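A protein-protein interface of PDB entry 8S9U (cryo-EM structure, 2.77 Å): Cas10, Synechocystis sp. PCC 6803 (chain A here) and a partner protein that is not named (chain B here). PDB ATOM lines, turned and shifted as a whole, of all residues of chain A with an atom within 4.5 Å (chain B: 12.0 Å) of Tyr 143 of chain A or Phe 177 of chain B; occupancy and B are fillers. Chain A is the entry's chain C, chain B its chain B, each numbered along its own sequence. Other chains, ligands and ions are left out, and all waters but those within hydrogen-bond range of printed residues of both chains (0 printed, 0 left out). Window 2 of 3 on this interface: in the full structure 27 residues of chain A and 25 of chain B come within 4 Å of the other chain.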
ATOM      1  N   PHE A  19     -21.403 -21.515 -19.461  1.00  0.00           N
ATOM      2  CA  PHE A  19     -21.386 -20.449 -20.444  1.00  0.00           C
ATOM      3  C   PHE A  19     -20.463 -19.347 -19.953  1.00  0.00           C
ATOM      4  O   PHE A  19     -20.368 -19.089 -18.752  1.00  0.00           O
ATOM      5  CB  PHE A  19     -22.794 -19.906 -20.681  1.00  0.00           C
ATOM      6  CG  PHE A  19     -23.714 -20.897 -21.324  1.00  0.00           C
ATOM      7  CD1 PHE A  19     -24.387 -21.825 -20.557  1.00  0.00           C
ATOM      8  CD2 PHE A  19     -23.891 -20.912 -22.691  1.00  0.00           C
ATOM      9  CE1 PHE A  19     -25.223 -22.744 -21.142  1.00  0.00           C
ATOM     10  CE2 PHE A  19     -24.726 -21.827 -23.279  1.00  0.00           C
ATOM     11  CZ  PHE A  19     -25.394 -22.744 -22.505  1.00  0.00           C
ATOM     12  N   LEU A  20     -19.785 -18.697 -20.885  1.00  0.00           N
ATOM     13  CA  LEU A  20     -19.014 -17.504 -20.582  1.00  0.00           C
ATOM     14  C   LEU A  20     -19.760 -16.272 -21.060  1.00  0.00           C
ATOM     15  O   LEU A  20     -20.125 -16.182 -22.234  1.00  0.00           O
ATOM     16  CB  LEU A  20     -17.636 -17.572 -21.236  1.00  0.00           C
ATOM     17  CG  LEU A  20     -16.737 -16.372 -20.980  1.00  0.00           C
ATOM     18  CD1 LEU A  20     -15.360 -16.841 -20.614  1.00  0.00           C
ATOM     19  CD2 LEU A  20     -16.680 -15.504 -22.211  1.00  0.00           C
ATOM     20  N   VAL A  21     -19.956 -15.319 -20.159  1.00  0.00           N
ATOM     21  CA  VAL A  21     -20.601 -14.054 -20.473  1.00  0.00           C
ATOM     22  C   VAL A  21     -19.522 -13.006 -20.664  1.00  0.00           C
ATOM     23  O   VAL A  21     -18.650 -12.844 -19.807  1.00  0.00           O
ATOM     24  CB  VAL A  21     -21.572 -13.642 -19.359  1.00  0.00           C
ATOM     25  CG1 VAL A  21     -22.042 -12.231 -19.574  1.00  0.00           C
ATOM     26  CG2 VAL A  21     -22.738 -14.600 -19.301  1.00  0.00           C
ATOM     27  N   GLU A 116     -27.815 -21.241 -19.178  1.00  0.00           N
ATOM     28  CA  GLU A 116     -28.000 -20.315 -20.290  1.00  0.00           C
ATOM     29  C   GLU A 116     -29.046 -19.255 -19.973  1.00  0.00           C
ATOM     30  O   GLU A 116     -28.867 -18.081 -20.316  1.00  0.00           O
ATOM     31  CB  GLU A 116     -28.390 -21.082 -21.551  1.00  0.00           C
ATOM     32  CG  GLU A 116     -28.236 -20.278 -22.828  1.00  0.00           C
ATOM     33  CD  GLU A 116     -28.697 -21.035 -24.056  1.00  0.00           C
ATOM     34  OE1 GLU A 116     -29.044 -20.384 -25.062  1.00  0.00           O
ATOM     35  OE2 GLU A 116     -28.714 -22.283 -24.019  1.00  0.00           O
ATOM     36  N   ALA A 119     -27.563 -16.685 -17.945  1.00  0.00           N
ATOM     37  CA  ALA A 119     -26.680 -15.891 -18.792  1.00  0.00           C
ATOM     38  C   ALA A 119     -27.446 -14.821 -19.556  1.00  0.00           C
ATOM     39  O   ALA A 119     -26.982 -13.682 -19.671  1.00  0.00           O
ATOM     40  CB  ALA A 119     -25.934 -16.799 -19.768  1.00  0.00           C
ATOM     41  N   LYS A 120     -28.612 -15.172 -20.099  1.00  0.00           N
ATOM     42  CA  LYS A 120     -29.458 -14.180 -20.754  1.00  0.00           C
ATOM     43  C   LYS A 120     -29.954 -13.134 -19.768  1.00  0.00           C
ATOM     44  O   LYS A 120     -29.891 -11.930 -20.035  1.00  0.00           O
ATOM     45  CB  LYS A 120     -30.644 -14.855 -21.435  1.00  0.00           C
ATOM     46  CG  LYS A 120     -31.298 -13.966 -22.471  1.00  0.00           C
ATOM     47  CD  LYS A 120     -32.565 -14.566 -23.055  1.00  0.00           C
ATOM     48  CE  LYS A 120     -33.695 -14.554 -22.037  1.00  0.00           C
ATOM     49  NZ  LYS A 120     -35.028 -14.489 -22.699  1.00  0.00           N
ATOM     50  N   ILE A 123     -27.347 -10.487 -18.833  1.00  0.00           N
ATOM     51  CA  ILE A 123     -27.096  -9.476 -19.856  1.00  0.00           C
ATOM     52  C   ILE A 123     -28.287  -8.541 -19.992  1.00  0.00           C
ATOM     53  O   ILE A 123     -28.124  -7.328 -20.161  1.00  0.00           O
ATOM     54  CB  ILE A 123     -26.741 -10.138 -21.199  1.00  0.00           C
ATOM     55  CG1 ILE A 123     -25.423 -10.900 -21.091  1.00  0.00           C
ATOM     56  CG2 ILE A 123     -26.618  -9.094 -22.279  1.00  0.00           C
ATOM     57  CD1 ILE A 123     -25.180 -11.840 -22.231  1.00  0.00           C
ATOM     58  N   GLY A 141     -23.846  -7.298 -24.497  1.00  0.00           N
ATOM     59  CA  GLY A 141     -23.203  -8.490 -23.993  1.00  0.00           C
ATOM     60  C   GLY A 141     -23.429  -9.678 -24.895  1.00  0.00           C
ATOM     61  O   GLY A 141     -24.282  -9.672 -25.781  1.00  0.00           O
ATOM     62  N   ILE A 142     -22.644 -10.716 -24.635  1.00  0.00           N
ATOM     63  CA  ILE A 142     -22.679 -11.965 -25.377  1.00  0.00           C
ATOM     64  C   ILE A 142     -22.465 -13.094 -24.385  1.00  0.00           C
ATOM     65  O   ILE A 142     -21.873 -12.899 -23.321  1.00  0.00           O
ATOM     66  CB  ILE A 142     -21.598 -11.961 -26.485  1.00  0.00           C
ATOM     67  CG1 ILE A 142     -21.643 -13.221 -27.340  1.00  0.00           C
ATOM     68  CG2 ILE A 142     -20.228 -11.797 -25.890  1.00  0.00           C
ATOM     69  CD1 ILE A 142     -22.937 -13.440 -28.003  1.00  0.00           C
ATOM     70  N   TYR A 143     -22.957 -14.277 -24.718  1.00  0.00           N
ATOM     71  CA  TYR A 143     -22.543 -15.477 -24.015  1.00  0.00           C
ATOM     72  C   TYR A 143     -22.216 -16.575 -25.013  1.00  0.00           C
ATOM     73  O   TYR A 143     -22.760 -16.614 -26.117  1.00  0.00           O
ATOM     74  CB  TYR A 143     -23.597 -15.936 -22.994  1.00  0.00           C
ATOM     75  CG  TYR A 143     -24.918 -16.414 -23.548  1.00  0.00           C
ATOM     76  CD1 TYR A 143     -25.025 -17.622 -24.212  1.00  0.00           C
ATOM     77  CD2 TYR A 143     -26.067 -15.667 -23.369  1.00  0.00           C
ATOM     78  CE1 TYR A 143     -26.228 -18.052 -24.711  1.00  0.00           C
ATOM     79  CE2 TYR A 143     -27.275 -16.095 -23.855  1.00  0.00           C
ATOM     80  CZ  TYR A 143     -27.350 -17.288 -24.526  1.00  0.00           C
ATOM     81  OH  TYR A 143     -28.556 -17.726 -25.012  1.00  0.00           O
ATOM     82  N   VAL A 144     -21.309 -17.466 -24.613  1.00  0.00           N
ATOM     83  CA  VAL A 144     -20.823 -18.542 -25.467  1.00  0.00           C
ATOM     84  C   VAL A 144     -20.676 -19.795 -24.618  1.00  0.00           C
ATOM     85  O   VAL A 144     -20.500 -19.723 -23.400  1.00  0.00           O
ATOM     86  CB  VAL A 144     -19.482 -18.205 -26.147  1.00  0.00           C
ATOM     87  CG1 VAL A 144     -19.596 -16.948 -26.972  1.00  0.00           C
ATOM     88  CG2 VAL A 144     -18.391 -18.062 -25.116  1.00  0.00           C
ATOM     89  N   ASN A 168     -22.174  -9.580 -33.511  1.00  0.00           N
ATOM     90  CA  ASN A 168     -23.542  -9.276 -33.118  1.00  0.00           C
ATOM     91  C   ASN A 168     -23.787  -7.789 -32.903  1.00  0.00           C
ATOM     92  O   ASN A 168     -24.938  -7.354 -32.984  1.00  0.00           O
ATOM     93  CB  ASN A 168     -23.895 -10.038 -31.847  1.00  0.00           C
ATOM     94  CG  ASN A 168     -24.191 -11.489 -32.109  1.00  0.00           C
ATOM     95  OD1 ASN A 168     -25.305 -11.845 -32.485  1.00  0.00           O
ATOM     96  ND2 ASN A 168     -23.196 -12.341 -31.919  1.00  0.00           N
ATOM     97  N   ILE B 115     -40.253  -4.284 -21.591  1.00  0.00           N
ATOM     98  CA  ILE B 115     -39.900  -4.499 -20.191  1.00  0.00           C
ATOM     99  C   ILE B 115     -40.368  -3.337 -19.325  1.00  0.00           C
ATOM    100  O   ILE B 115     -41.017  -3.535 -18.294  1.00  0.00           O
ATOM    101  CB  ILE B 115     -38.387  -4.734 -20.053  1.00  0.00           C
ATOM    102  CG1 ILE B 115     -37.998  -6.036 -20.749  1.00  0.00           C
ATOM    103  CG2 ILE B 115     -37.980  -4.755 -18.598  1.00  0.00           C
ATOM    104  CD1 ILE B 115     -36.560  -6.104 -21.138  1.00  0.00           C
ATOM    105  N   ALA B 172     -37.134  -3.142 -24.558  1.00  0.00           N
ATOM    106  CA  ALA B 172     -37.389  -4.564 -24.717  1.00  0.00           C
ATOM    107  C   ALA B 172     -36.106  -5.268 -25.126  1.00  0.00           C
ATOM    108  O   ALA B 172     -35.154  -4.642 -25.595  1.00  0.00           O
ATOM    109  CB  ALA B 172     -38.484  -4.827 -25.750  1.00  0.00           C
ATOM    110  N   GLU B 173     -36.094  -6.585 -24.937  1.00  0.00           N
ATOM    111  CA  GLU B 173     -34.984  -7.402 -25.407  1.00  0.00           C
ATOM    112  C   GLU B 173     -34.976  -7.455 -26.925  1.00  0.00           C
ATOM    113  O   GLU B 173     -35.978  -7.818 -27.548  1.00  0.00           O
ATOM    114  CB  GLU B 173     -35.077  -8.817 -24.849  1.00  0.00           C
ATOM    115  CG  GLU B 173     -35.138  -8.896 -23.348  1.00  0.00           C
ATOM    116  CD  GLU B 173     -35.660 -10.226 -22.883  1.00  0.00           C
ATOM    117  OE1 GLU B 173     -36.342 -10.267 -21.841  1.00  0.00           O
ATOM    118  OE2 GLU B 173     -35.389 -11.233 -23.568  1.00  0.00           O
ATOM    119  N   VAL B 174     -33.839  -7.114 -27.520  1.00  0.00           N
ATOM    120  CA  VAL B 174     -33.681  -7.247 -28.959  1.00  0.00           C
ATOM    121  C   VAL B 174     -33.054  -8.590 -29.307  1.00  0.00           C
ATOM    122  O   VAL B 174     -33.644  -9.393 -30.036  1.00  0.00           O
ATOM    123  CB  VAL B 174     -32.828  -6.094 -29.505  1.00  0.00           C
ATOM    124  CG1 VAL B 174     -32.511  -6.322 -30.969  1.00  0.00           C
ATOM    125  CG2 VAL B 174     -33.541  -4.776 -29.295  1.00  0.00           C
ATOM    126  N   ASP B 175     -31.866  -8.848 -28.774  1.00  0.00           N
ATOM    127  CA  ASP B 175     -31.148 -10.077 -29.064  1.00  0.00           C
ATOM    128  C   ASP B 175     -31.626 -11.227 -28.190  1.00  0.00           C
ATOM    129  O   ASP B 175     -32.174 -11.029 -27.103  1.00  0.00           O
ATOM    130  CB  ASP B 175     -29.644  -9.878 -28.890  1.00  0.00           C
ATOM    131  CG  ASP B 175     -29.070  -8.893 -29.886  1.00  0.00           C
ATOM    132  OD1 ASP B 175     -29.747  -8.609 -30.895  1.00  0.00           O
ATOM    133  OD2 ASP B 175     -27.934  -8.418 -29.679  1.00  0.00           O
ATOM    134  N   ASP B 176     -31.437 -12.445 -28.697  1.00  0.00           N
ATOM    135  CA  ASP B 176     -31.655 -13.628 -27.877  1.00  0.00           C
ATOM    136  C   ASP B 176     -30.651 -13.732 -26.740  1.00  0.00           C
ATOM    137  O   ASP B 176     -30.913 -14.436 -25.761  1.00  0.00           O
ATOM    138  CB  ASP B 176     -31.584 -14.891 -28.732  1.00  0.00           C
ATOM    139  CG  ASP B 176     -32.639 -14.921 -29.815  1.00  0.00           C
ATOM    140  OD1 ASP B 176     -33.589 -14.117 -29.741  1.00  0.00           O
ATOM    141  OD2 ASP B 176     -32.524 -15.759 -30.733  1.00  0.00           O
ATOM    142  N   PHE B 177     -29.504 -13.062 -26.851  1.00  0.00           N
ATOM    143  CA  PHE B 177     -28.582 -12.905 -25.735  1.00  0.00           C
ATOM    144  C   PHE B 177     -29.093 -11.939 -24.678  1.00  0.00           C
ATOM    145  O   PHE B 177     -28.380 -11.688 -23.702  1.00  0.00           O
ATOM    146  CB  PHE B 177     -27.223 -12.437 -26.247  1.00  0.00           C
ATOM    147  CG  PHE B 177     -26.675 -13.296 -27.335  1.00  0.00           C
ATOM    148  CD1 PHE B 177     -26.363 -14.618 -27.101  1.00  0.00           C
ATOM    149  CD2 PHE B 177     -26.467 -12.780 -28.597  1.00  0.00           C
ATOM    150  CE1 PHE B 177     -25.870 -15.411 -28.106  1.00  0.00           C
ATOM    151  CE2 PHE B 177     -25.971 -13.570 -29.604  1.00  0.00           C
ATOM    152  CZ  PHE B 177     -25.672 -14.888 -29.357  1.00  0.00           C
ATOM    153  N   GLY B 178     -30.285 -11.382 -24.851  1.00  0.00           N
ATOM    154  CA  GLY B 178     -30.931 -10.613 -23.817  1.00  0.00           C
ATOM    155  C   GLY B 178     -30.627  -9.136 -23.827  1.00  0.00           C
ATOM    156  O   GLY B 178     -31.149  -8.414 -22.974  1.00  0.00           O
ATOM    157  N   ASN B 179     -29.808  -8.663 -24.758  1.00  0.00           N
ATOM    158  CA  ASN B 179     -29.518  -7.240 -24.870  1.00  0.00           C
ATOM    159  C   ASN B 179     -30.792  -6.420 -24.989  1.00  0.00           C
ATOM    160  O   ASN B 179     -31.577  -6.605 -25.922  1.00  0.00           O
ATOM    161  CB  ASN B 179     -28.625  -7.001 -26.082  1.00  0.00           C
ATOM    162  CG  ASN B 179     -27.245  -7.550 -25.893  1.00  0.00           C
ATOM    163  OD1 ASN B 179     -26.508  -7.110 -25.020  1.00  0.00           O
ATOM    164  ND2 ASN B 179     -26.885  -8.530 -26.703  1.00  0.00           N
ATOM    165  N   CYS B 180     -30.996  -5.518 -24.037  1.00  0.00           N
ATOM    166  CA  CYS B 180     -32.120  -4.599 -24.082  1.00  0.00           C
ATOM    167  C   CYS B 180     -31.809  -3.407 -24.975  1.00  0.00           C
ATOM    168  O   CYS B 180     -30.653  -3.010 -25.136  1.00  0.00           O
ATOM    169  CB  CYS B 180     -32.477  -4.125 -22.678  1.00  0.00           C
ATOM    170  SG  CYS B 180     -33.148  -5.433 -21.640  1.00  0.00           S
ATOM    171  N   ALA B 181     -32.861  -2.836 -25.557  1.00  0.00           N
ATOM    172  CA  ALA B 181     -32.783  -1.542 -26.220  1.00  0.00           C
ATOM    173  C   ALA B 181     -34.146  -0.881 -26.125  1.00  0.00           C
ATOM    174  O   ALA B 181     -35.146  -1.536 -25.831  1.00  0.00           O
ATOM    175  CB  ALA B 181     -32.347  -1.671 -27.682  1.00  0.00           C
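Printed residues of chain A that touch a printed residue of chain B: Lys 120, Ile 123, Gly 141, Ile 142, Tyr 143 and Asn 168.
Hydrophobic or aromatic side chains of chain A within 4 Å of the printed part of chain B: Ile 123, Ile 142 and Tyr 143.
Printed residues of chain B that touch a printed residue of chain A: Glu 173, Asp 176, Phe 177, Gly 178 and Asn 179.
Hydrophobic or aromatic side chains of chain B that line the printed part of chain A: Phe 177.
Among the printed residues, 10 pairs touch across the chains.
N of Val 174 of chain B is in hydrogen-bond range of O of Asn 179 of chain B, at 2.8 Å.
The side-chain carboxylate (OD2) of Asp 175 of chain B is in hydrogen-bond range of the side-chain amide nitrogen (ND2) of Asn 179 of chain B, at 3.2 Å.
The side-chain carboxylate (OE1) of Glu 116 of chain A is in hydrogen-bond range of the side-chain hydroxyl (OH) of Tyr 143 of chain A (2.7 Å).
Tyr 143 of chain A touches just one residue of chain B: Phe 177 (3.7 Å).
Of chain A, only Lys 120 (3.7 Å), Ile 123 (3.4 Å), Ile 142 (3.4 Å), Tyr 143 (3.7 Å) and Asn 168 (3.4 Å) come within 4 Å of Phe 177 of chain B.
No residue of chain B comes within 4 Å of Phe 19 of chain A.
No residue of chain B comes within 4 Å of Val 21 of chain A.
No residue of chain B comes within 4 Å of Glu 116 of chain A.
No residue of chain B comes within 4 Å of Ala 119 of chain A.
Of chain B, only Glu 173 (3.4 Å), Asp 176 (3.2 Å), Phe 177 (3.7 Å) and Gly 178 (3.6 Å) come within 4 Å of Lys 120 of chain A.
Of the printed residues of chain B, Gly 141 of chain A touches Asn 179 (2.7 Å).
Ile 142 of chain A touches just one residue of chain B: Phe 177 (3.4 Å).
No residue of chain B comes within 4 Å of Val 144 of chain A.
Of chain B, only Phe 177 comes within 4 Å of Asn 168 of chain A.
Of the printed residues of chain A, Asp 176 of chain B touches Lys 120.
Of the printed residues of chain A, Asn 179 of chain B touches Ile 123 and Gly 141.
Cys 180 of chain B touches none of the printed residues of chain A.
Leu 20 of chain A touches none of the printed residues of chain B.
The nearest residue of chain B that does not touch Tyr 143 of chain A is Asp 176 of chain B (4.1 Å).
The nearest residue of chain A that does not touch Phe 177 of chain B is Gly 141 of chain A (4.1 Å).
Among the printed residues, pairs that only touch across the chains: Lys 120 of chain A with Asp 176 of chain B, Lys 120 of chain A with Phe 177 of chain B, Lys 120 of chain A with Gly 178 of chain B, Ile 123 of chain A with Phe 177 of chain B, Ile 123 of chain A with Asn 179 of chain B, Ile 142 of chain A with Phe 177 of chain B, Tyr 143 of chain A with Phe 177 of chain B and Asn 168 of chain A with Phe 177 of chain B.
The side-chain amide oxygen of Asn 179 of chain B lies within hydrogen-bond range of the backbone NH of Gly 141 of chain A, at 2.7 Å.
OE2 of Glu 173 of chain B lies within salt-bridge range of NZ of Lys 120 of chain A, at 3.4 Å.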
